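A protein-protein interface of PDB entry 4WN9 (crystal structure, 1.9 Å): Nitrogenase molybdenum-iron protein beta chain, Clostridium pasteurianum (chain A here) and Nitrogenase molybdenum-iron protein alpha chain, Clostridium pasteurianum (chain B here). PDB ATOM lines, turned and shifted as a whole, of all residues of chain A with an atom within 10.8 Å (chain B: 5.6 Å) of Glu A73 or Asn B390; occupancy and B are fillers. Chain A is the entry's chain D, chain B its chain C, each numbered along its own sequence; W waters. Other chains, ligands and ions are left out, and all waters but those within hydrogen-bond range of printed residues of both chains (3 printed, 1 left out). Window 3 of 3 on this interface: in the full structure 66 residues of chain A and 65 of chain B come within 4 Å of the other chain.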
ATOM      1  N   GLY A  44     -11.491 -11.477  -3.022  1.00  0.00           N
ATOM      2  CA  GLY A  44     -10.316 -12.312  -2.987  1.00  0.00           C
ATOM      3  C   GLY A  44     -10.688 -13.623  -2.359  1.00  0.00           C
ATOM      4  O   GLY A  44     -11.870 -13.976  -2.325  1.00  0.00           O
ATOM      5  N   SER A  45      -9.687 -14.345  -1.868  1.00  0.00           N
ATOM      6  CA  SER A  45      -9.950 -15.582  -1.169  1.00  0.00           C
ATOM      7  C   SER A  45     -10.369 -15.262   0.264  1.00  0.00           C
ATOM      8  O   SER A  45      -9.882 -14.304   0.866  1.00  0.00           O
ATOM      9  CB  SER A  45      -8.747 -16.488  -1.191  1.00  0.00           C
ATOM     10  OG  SER A  45      -8.886 -17.462  -0.188  1.00  0.00           O
ATOM     11  N   GLN A  46     -11.286 -16.061   0.782  1.00  0.00           N
ATOM     12  CA  GLN A  46     -12.033 -15.711   1.985  1.00  0.00           C
ATOM     13  C   GLN A  46     -11.145 -15.611   3.238  1.00  0.00           C
ATOM     14  O   GLN A  46     -11.550 -15.026   4.241  1.00  0.00           O
ATOM     15  CB  GLN A  46     -13.177 -16.717   2.188  1.00  0.00           C
ATOM     16  CG  GLN A  46     -12.707 -18.124   2.509  1.00  0.00           C
ATOM     17  CD  GLN A  46     -13.698 -19.198   2.141  1.00  0.00           C
ATOM     18  OE1 GLN A  46     -14.872 -18.935   1.880  1.00  0.00           O
ATOM     19  NE2 GLN A  46     -13.227 -20.434   2.138  1.00  0.00           N
ATOM     20  N   SER A  69     -15.752 -12.637  -1.878  1.00  0.00           N
ATOM     21  CA  SER A  69     -16.026 -13.309  -3.144  1.00  0.00           C
ATOM     22  C   SER A  69     -15.706 -14.793  -3.056  1.00  0.00           C
ATOM     23  O   SER A  69     -16.094 -15.571  -3.919  1.00  0.00           O
ATOM     24  CB  SER A  69     -15.193 -12.690  -4.263  1.00  0.00           C
ATOM     25  OG  SER A  69     -15.640 -11.382  -4.565  1.00  0.00           O
ATOM     26  N   SER A  70     -14.979 -15.162  -2.017  1.00  0.00           N
ATOM     27  CA  SER A  70     -14.524 -16.540  -1.800  1.00  0.00           C
ATOM     28  C   SER A  70     -13.915 -17.225  -3.048  1.00  0.00           C
ATOM     29  O   SER A  70     -14.360 -18.295  -3.460  1.00  0.00           O
ATOM     30  CB  SER A  70     -15.670 -17.373  -1.217  1.00  0.00           C
ATOM     31  OG  SER A  70     -15.992 -16.940   0.099  1.00  0.00           O
ATOM     32  N   PHE A  71     -12.858 -16.633  -3.600  1.00  0.00           N
ATOM     33  CA  PHE A  71     -12.119 -17.236  -4.717  1.00  0.00           C
ATOM     34  C   PHE A  71     -11.770 -18.688  -4.454  1.00  0.00           C
ATOM     35  O   PHE A  71     -11.344 -19.045  -3.361  1.00  0.00           O
ATOM     36  CB  PHE A  71     -10.799 -16.508  -4.961  1.00  0.00           C
ATOM     37  CG  PHE A  71     -10.889 -15.357  -5.913  1.00  0.00           C
ATOM     38  CD1 PHE A  71     -11.733 -14.294  -5.663  1.00  0.00           C
ATOM     39  CD2 PHE A  71     -10.064 -15.305  -7.028  1.00  0.00           C
ATOM     40  CE1 PHE A  71     -11.802 -13.224  -6.537  1.00  0.00           C
ATOM     41  CE2 PHE A  71     -10.123 -14.232  -7.913  1.00  0.00           C
ATOM     42  CZ  PHE A  71     -10.990 -13.187  -7.662  1.00  0.00           C
ATOM     43  N   THR A  72     -11.977 -19.514  -5.472  1.00  0.00           N
ATOM     44  CA  THR A  72     -11.459 -20.866  -5.518  1.00  0.00           C
ATOM     45  C   THR A  72     -10.339 -20.860  -6.552  1.00  0.00           C
ATOM     46  O   THR A  72     -10.119 -19.833  -7.207  1.00  0.00           O
ATOM     47  CB  THR A  72     -12.553 -21.846  -5.962  1.00  0.00           C
ATOM     48  OG1 THR A  72     -13.335 -21.238  -6.990  1.00  0.00           O
ATOM     49  CG2 THR A  72     -13.459 -22.202  -4.799  1.00  0.00           C
ATOM     50  N   GLU A  73      -9.631 -21.984  -6.687  1.00  0.00           N
ATOM     51  CA  GLU A  73      -8.455 -22.046  -7.562  1.00  0.00           C
ATOM     52  C   GLU A  73      -8.820 -21.703  -9.005  1.00  0.00           C
ATOM     53  O   GLU A  73      -8.055 -21.033  -9.711  1.00  0.00           O
ATOM     54  CB  GLU A  73      -7.812 -23.439  -7.504  1.00  0.00           C
ATOM     55  CG  GLU A  73      -6.653 -23.651  -8.471  1.00  0.00           C
ATOM     56  CD  GLU A  73      -5.749 -24.793  -8.053  1.00  0.00           C
ATOM     57  OE1 GLU A  73      -6.250 -25.762  -7.445  1.00  0.00           O
ATOM     58  OE2 GLU A  73      -4.532 -24.722  -8.316  1.00  0.00           O
ATOM     59  N   GLY A  74      -9.994 -22.155  -9.430  1.00  0.00           N
ATOM     60  CA  GLY A  74     -10.496 -21.904 -10.787  1.00  0.00           C
ATOM     61  C   GLY A  74     -10.599 -20.425 -11.083  1.00  0.00           C
ATOM     62  O   GLY A  74     -10.069 -19.932 -12.089  1.00  0.00           O
ATOM     63  N   ALA A  75     -11.284 -19.702 -10.202  1.00  0.00           N
ATOM     64  CA  ALA A  75     -11.434 -18.267 -10.374  1.00  0.00           C
ATOM     65  C   ALA A  75     -10.086 -17.565 -10.209  1.00  0.00           C
ATOM     66  O   ALA A  75      -9.872 -16.504 -10.782  1.00  0.00           O
ATOM     67  CB  ALA A  75     -12.467 -17.714  -9.402  1.00  0.00           C
ATOM     68  N   SER A  76      -9.162 -18.177  -9.463  1.00  0.00           N
ATOM     69  CA  SER A  76      -7.879 -17.534  -9.190  1.00  0.00           C
ATOM     70  C   SER A  76      -6.917 -17.622 -10.386  1.00  0.00           C
ATOM     71  O   SER A  76      -5.861 -16.962 -10.406  1.00  0.00           O
ATOM     72  CB  SER A  76      -7.242 -18.123  -7.920  1.00  0.00           C
ATOM     73  OG  SER A  76      -7.990 -17.766  -6.756  1.00  0.00           O
ATOM     74  N   VAL A  77      -7.282 -18.423 -11.378  1.00  0.00           N
ATOM     75  CA  VAL A  77      -6.492 -18.522 -12.595  1.00  0.00           C
ATOM     76  C   VAL A  77      -7.191 -17.805 -13.750  1.00  0.00           C
ATOM     77  O   VAL A  77      -6.552 -17.106 -14.536  1.00  0.00           O
ATOM     78  CB  VAL A  77      -6.226 -19.993 -12.942  1.00  0.00           C
ATOM     79  CG1 VAL A  77      -5.443 -20.113 -14.242  1.00  0.00           C
ATOM     80  CG2 VAL A  77      -5.468 -20.656 -11.810  1.00  0.00           C
ATOM     81  N   PHE A  78      -8.511 -17.934 -13.841  1.00  0.00           N
ATOM     82  CA  PHE A  78      -9.217 -17.432 -15.019  1.00  0.00           C
ATOM     83  C   PHE A  78     -10.063 -16.198 -14.772  1.00  0.00           C
ATOM     84  O   PHE A  78     -10.714 -15.713 -15.689  1.00  0.00           O
ATOM     85  CB  PHE A  78     -10.053 -18.558 -15.641  1.00  0.00           C
ATOM     86  CG  PHE A  78      -9.227 -19.744 -16.037  1.00  0.00           C
ATOM     87  CD1 PHE A  78      -8.377 -19.675 -17.141  1.00  0.00           C
ATOM     88  CD2 PHE A  78      -9.268 -20.920 -15.300  1.00  0.00           C
ATOM     89  CE1 PHE A  78      -7.589 -20.753 -17.500  1.00  0.00           C
ATOM     90  CE2 PHE A  78      -8.487 -22.008 -15.658  1.00  0.00           C
ATOM     91  CZ  PHE A  78      -7.648 -21.925 -16.758  1.00  0.00           C
ATOM     92  N   GLY A  79     -10.041 -15.670 -13.552  1.00  0.00           N
ATOM     93  CA  GLY A  79     -10.760 -14.434 -13.256  1.00  0.00           C
ATOM     94  C   GLY A  79     -11.891 -14.648 -12.277  1.00  0.00           C
ATOM     95  O   GLY A  79     -12.467 -15.733 -12.218  1.00  0.00           O
ATOM     96  N   GLY A  80     -12.217 -13.602 -11.523  1.00  0.00           N
ATOM     97  CA  GLY A  80     -13.167 -13.706 -10.426  1.00  0.00           C
ATOM     98  C   GLY A  80     -14.483 -13.010 -10.679  1.00  0.00           C
ATOM     99  O   GLY A  80     -15.179 -12.634  -9.738  1.00  0.00           O
ATOM    100  N   SER A  82     -17.465 -14.108 -12.048  1.00  0.00           N
ATOM    101  CA  SER A  82     -18.679 -14.794 -11.609  1.00  0.00           C
ATOM    102  C   SER A  82     -18.782 -14.735 -10.075  1.00  0.00           C
ATOM    103  O   SER A  82     -19.845 -14.424  -9.531  1.00  0.00           O
ATOM    104  CB  SER A  82     -18.735 -16.245 -12.125  1.00  0.00           C
ATOM    105  OG  SER A  82     -17.562 -16.972 -11.794  1.00  0.00           O
ATOM    106  N   ASN A  83     -17.667 -14.980  -9.387  1.00  0.00           N
ATOM    107  CA  ASN A  83     -17.669 -14.936  -7.929  1.00  0.00           C
ATOM    108  C   ASN A  83     -18.295 -13.655  -7.411  1.00  0.00           C
ATOM    109  O   ASN A  83     -19.214 -13.706  -6.609  1.00  0.00           O
ATOM    110  CB  ASN A  83     -16.270 -15.097  -7.364  1.00  0.00           C
ATOM    111  CG  ASN A  83     -15.749 -16.511  -7.502  1.00  0.00           C
ATOM    112  OD1 ASN A  83     -15.631 -17.038  -8.611  1.00  0.00           O
ATOM    113  ND2 ASN A  83     -15.413 -17.129  -6.381  1.00  0.00           N
ATOM    114  N   LEU A 107      -4.463 -11.330  -4.476  1.00  0.00           N
ATOM    115  CA  LEU A 107      -4.950 -12.327  -5.422  1.00  0.00           C
ATOM    116  C   LEU A 107      -5.615 -11.697  -6.642  1.00  0.00           C
ATOM    117  O   LEU A 107      -5.168 -11.910  -7.769  1.00  0.00           O
ATOM    118  CB  LEU A 107      -5.943 -13.250  -4.703  1.00  0.00           C
ATOM    119  CG  LEU A 107      -6.514 -14.419  -5.503  1.00  0.00           C
ATOM    120  CD1 LEU A 107      -5.460 -15.035  -6.411  1.00  0.00           C
ATOM    121  CD2 LEU A 107      -7.087 -15.459  -4.548  1.00  0.00           C
ATOM    122  N   SER A 108      -6.672 -10.921  -6.424  1.00  0.00           N
ATOM    123  CA  SER A 108      -7.396 -10.299  -7.527  1.00  0.00           C
ATOM    124  C   SER A 108      -6.588  -9.220  -8.257  1.00  0.00           C
ATOM    125  O   SER A 108      -6.876  -8.913  -9.421  1.00  0.00           O
ATOM    126  CB  SER A 108      -8.732  -9.716  -7.051  1.00  0.00           C
ATOM    127  OG  SER A 108      -8.606  -9.039  -5.816  1.00  0.00           O
ATOM    128  N   LEU A 111      -3.973 -10.929 -10.474  1.00  0.00           N
ATOM    129  CA  LEU A 111      -4.738 -11.549 -11.549  1.00  0.00           C
ATOM    130  C   LEU A 111      -5.159 -10.499 -12.564  1.00  0.00           C
ATOM    131  O   LEU A 111      -5.386 -10.803 -13.731  1.00  0.00           O
ATOM    132  CB  LEU A 111      -6.003 -12.183 -10.965  1.00  0.00           C
ATOM    133  CG  LEU A 111      -6.326 -13.639 -11.294  1.00  0.00           C
ATOM    134  CD1 LEU A 111      -7.625 -14.034 -10.615  1.00  0.00           C
ATOM    135  CD2 LEU A 111      -6.422 -13.840 -12.792  1.00  0.00           C
ATOM    136  N   ASP A 113      -8.015  -8.637 -12.222  1.00  0.00           N
ATOM    137  CA  ASP A 113      -9.469  -8.519 -12.330  1.00  0.00           C
ATOM    138  C   ASP A 113      -9.862  -7.067 -12.612  1.00  0.00           C
ATOM    139  O   ASP A 113      -9.300  -6.146 -12.018  1.00  0.00           O
ATOM    140  CB  ASP A 113     -10.168  -9.006 -11.052  1.00  0.00           C
ATOM    141  CG  ASP A 113     -10.465 -10.502 -11.071  1.00  0.00           C
ATOM    142  OD1 ASP A 113      -9.873 -11.238 -11.899  1.00  0.00           O
ATOM    143  OD2 ASP A 113     -11.299 -10.939 -10.252  1.00  0.00           O
ATOM    144  N   TYR B 175      -6.095 -19.931  -2.078  1.00  0.00           N
ATOM    145  CA  TYR B 175      -7.238 -20.249  -2.928  1.00  0.00           C
ATOM    146  C   TYR B 175      -7.415 -21.756  -3.173  1.00  0.00           C
ATOM    147  O   TYR B 175      -8.348 -22.176  -3.866  1.00  0.00           O
ATOM    148  CB  TYR B 175      -7.108 -19.527  -4.273  1.00  0.00           C
ATOM    149  CG  TYR B 175      -5.791 -19.784  -4.975  1.00  0.00           C
ATOM    150  CD1 TYR B 175      -5.539 -20.986  -5.614  1.00  0.00           C
ATOM    151  CD2 TYR B 175      -4.800 -18.814  -4.997  1.00  0.00           C
ATOM    152  CE1 TYR B 175      -4.340 -21.212  -6.263  1.00  0.00           C
ATOM    153  CE2 TYR B 175      -3.600 -19.030  -5.635  1.00  0.00           C
ATOM    154  CZ  TYR B 175      -3.376 -20.227  -6.268  1.00  0.00           C
ATOM    155  OH  TYR B 175      -2.170 -20.437  -6.886  1.00  0.00           O
ATOM    156  N   LYS B 176      -6.513 -22.571  -2.641  1.00  0.00           N
ATOM    157  CA  LYS B 176      -6.588 -23.991  -2.908  1.00  0.00           C
ATOM    158  C   LYS B 176      -7.682 -24.595  -2.058  1.00  0.00           C
ATOM    159  O   LYS B 176      -7.860 -24.233  -0.883  1.00  0.00           O
ATOM    160  CB  LYS B 176      -5.253 -24.678  -2.635  1.00  0.00           C
ATOM    161  CG  LYS B 176      -4.178 -24.301  -3.658  1.00  0.00           C
ATOM    162  CD  LYS B 176      -2.936 -25.160  -3.535  1.00  0.00           C
ATOM    163  CE  LYS B 176      -1.900 -24.801  -4.593  1.00  0.00           C
ATOM    164  NZ  LYS B 176      -2.481 -24.709  -5.962  1.00  0.00           N
ATOM    165  N   GLY B 177      -8.415 -25.531  -2.645  1.00  0.00           N
ATOM    166  CA  GLY B 177      -9.480 -26.173  -1.908  1.00  0.00           C
ATOM    167  C   GLY B 177     -10.531 -25.119  -1.682  1.00  0.00           C
ATOM    168  O   GLY B 177     -10.659 -24.184  -2.469  1.00  0.00           O
ATOM    169  N   ALA B 386     -14.720 -30.564  -8.058  1.00  0.00           N
ATOM    170  CA  ALA B 386     -13.809 -29.755  -8.874  1.00  0.00           C
ATOM    171  C   ALA B 386     -12.933 -28.820  -8.039  1.00  0.00           C
ATOM    172  O   ALA B 386     -11.833 -28.469  -8.458  1.00  0.00           O
ATOM    173  CB  ALA B 386     -14.601 -28.941  -9.888  1.00  0.00           C
ATOM    174  N   ASP B 387     -13.408 -28.407  -6.865  1.00  0.00           N
ATOM    175  CA  ASP B 387     -12.714 -27.342  -6.150  1.00  0.00           C
ATOM    176  C   ASP B 387     -11.606 -27.870  -5.264  1.00  0.00           C
ATOM    177  O   ASP B 387     -10.764 -27.109  -4.769  1.00  0.00           O
ATOM    178  CB  ASP B 387     -13.713 -26.488  -5.373  1.00  0.00           C
ATOM    179  CG  ASP B 387     -14.661 -25.753  -6.281  1.00  0.00           C
ATOM    180  OD1 ASP B 387     -14.190 -25.058  -7.224  1.00  0.00           O
ATOM    181  OD2 ASP B 387     -15.884 -25.861  -6.055  1.00  0.00           O
ATOM    182  N   SER B 388     -11.578 -29.181  -5.077  1.00  0.00           N
ATOM    183  CA  SER B 388     -10.587 -29.766  -4.200  1.00  0.00           C
ATOM    184  C   SER B 388      -9.802 -30.887  -4.906  1.00  0.00           C
ATOM    185  O   SER B 388      -8.966 -31.561  -4.289  1.00  0.00           O
ATOM    186  CB  SER B 388     -11.267 -30.279  -2.916  1.00  0.00           C
ATOM    187  OG  SER B 388     -11.860 -29.218  -2.165  1.00  0.00           O
ATOM    188  N   LYS B 389     -10.063 -31.083  -6.198  1.00  0.00           N
ATOM    189  CA  LYS B 389      -9.419 -32.174  -6.929  1.00  0.00           C
ATOM    190  C   LYS B 389      -7.916 -31.942  -7.118  1.00  0.00           C
ATOM    191  O   LYS B 389      -7.163 -32.891  -7.296  1.00  0.00           O
ATOM    192  CB  LYS B 389     -10.114 -32.460  -8.272  1.00  0.00           C
ATOM    193  CG  LYS B 389     -10.280 -31.275  -9.205  1.00  0.00           C
ATOM    194  CD  LYS B 389     -11.039 -31.660 -10.474  1.00  0.00           C
ATOM    195  CE  LYS B 389     -11.253 -30.456 -11.387  1.00  0.00           C
ATOM    196  NZ  LYS B 389     -11.929 -30.792 -12.673  1.00  0.00           N
ATOM    197  N   ASN B 390      -7.477 -30.691  -7.053  1.00  0.00           N
ATOM    198  CA  ASN B 390      -6.057 -30.381  -7.217  1.00  0.00           C
ATOM    199  C   ASN B 390      -5.264 -30.453  -5.911  1.00  0.00           C
ATOM    200  O   ASN B 390      -4.069 -30.154  -5.895  1.00  0.00           O
ATOM    201  CB  ASN B 390      -5.876 -29.000  -7.855  1.00  0.00           C
ATOM    202  CG  ASN B 390      -6.404 -28.933  -9.287  1.00  0.00           C
ATOM    203  OD1 ASN B 390      -6.377 -29.920 -10.030  1.00  0.00           O
ATOM    204  ND2 ASN B 390      -6.875 -27.753  -9.684  1.00  0.00           N
ATOM    205  N   ILE B 391      -5.909 -30.854  -4.816  1.00  0.00           N
ATOM    206  CA  ILE B 391      -5.168 -31.132  -3.584  1.00  0.00           C
ATOM    207  C   ILE B 391      -4.444 -32.455  -3.768  1.00  0.00           C
ATOM    208  O   ILE B 391      -5.073 -33.473  -4.020  1.00  0.00           O
ATOM    209  CB  ILE B 391      -6.071 -31.219  -2.339  1.00  0.00           C
ATOM    210  CG1 ILE B 391      -7.062 -30.051  -2.298  1.00  0.00           C
ATOM    211  CG2 ILE B 391      -5.230 -31.208  -1.076  1.00  0.00           C
ATOM    212  CD1 ILE B 391      -6.399 -28.708  -2.501  1.00  0.00           C
ATOM    213  N   PRO B 392      -3.109 -32.443  -3.667  1.00  0.00           N
ATOM    214  CA  PRO B 392      -2.374 -33.670  -3.948  1.00  0.00           C
ATOM    215  C   PRO B 392      -2.637 -34.793  -2.955  1.00  0.00           C
ATOM    216  O   PRO B 392      -2.586 -34.590  -1.726  1.00  0.00           O
ATOM    217  CB  PRO B 392      -0.901 -33.241  -3.883  1.00  0.00           C
ATOM    218  CG  PRO B 392      -0.898 -31.887  -3.262  1.00  0.00           C
ATOM    219  CD  PRO B 392      -2.223 -31.274  -3.574  1.00  0.00           C
HETATM  220  O   HOH W   1     -11.661 -21.452  -1.986  1.00  0.00           O
HETATM  221  O   HOH W   2      -7.517 -26.384  -5.252  1.00  0.00           O
HETATM  222  O   HOH W   3     -11.625 -24.365  -8.325  1.00  0.00           O
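Glu A73 touches just these residues of chain B: Tyr B175, Lys B176 and Asn B390. Of chain A, only Glu A73 (3.1 Å) comes within 4 Å of Asn B390. Of chain A, only Glu A73 (3.1 Å) comes within 4 Å of Lys B176. No residue of chain A comes within 4 Å of Ser B388. No residue of chain A comes within 4 Å of Lys B389. No residue of chain A comes within 4 Å of Ile B391. No residue of chain A comes within 4 Å of Pro B392. Of the printed residues of chain B, Ser A76 touches Tyr B175 (3.2 Å). Printed residues of chain A within 4 Å of Tyr B175: Thr A72 (3.6 Å), Glu A73 (3.1 Å) and Ser A76 (3.2 Å). Of the printed residues of chain B, Thr A72 touches Tyr B175 (3.6 Å) and Asp B387 (3.8 Å). The nearest residue of chain A that does not touch Asn B390 is Gly A74 (6.4 Å). The nearest printed residue of chain B that does not touch Thr A72 is Gly B177 (4.1 Å).
ND2 of Asn B390 is in hydrogen-bond range of OE1 of Glu A73 (3.1 Å). NZ of Lys B176 lies within salt-bridge range of OE2 of Glu A73 (3.1 Å). O of Tyr B175 lies within hydrogen-bond range of N of Glu A73, 3.1 Å away.
Water W2 lies within hydrogen-bond range of OE1 of Glu A73 (2.6 Å), N of Gly B177 (2.9 Å) and O of Asp B387 (3.4 Å). Water W1 bridges O of Phe A71 (2.8 Å) and O of Gly B177 (2.9 Å). Water W3 bridges the side-chain carboxylate of Asp B387 and the backbone NH of Gly A74.
Printed residues of chain A that touch a printed residue of chain B: Thr A72, Glu A73 and Ser A76. Printed residues of chain B that touch a printed residue of chain A: Tyr B175, Lys B176, Asp B387 and Asn B390. Hydrophobic or aromatic side chains of chain B that line the printed part of chain A: Tyr B175. Among the printed residues, 6 pairs touch across the chains.
O of Thr A72 is in hydrogen-bond range of OG of Ser A76, at 3.0 Å.
Among the printed residues, merely in contact across the chains: Thr A72 with Tyr B175 (3.6 Å), Thr A72 with Asp B387 (3.8 Å) and Ser A76 with Tyr B175 (3.2 Å).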
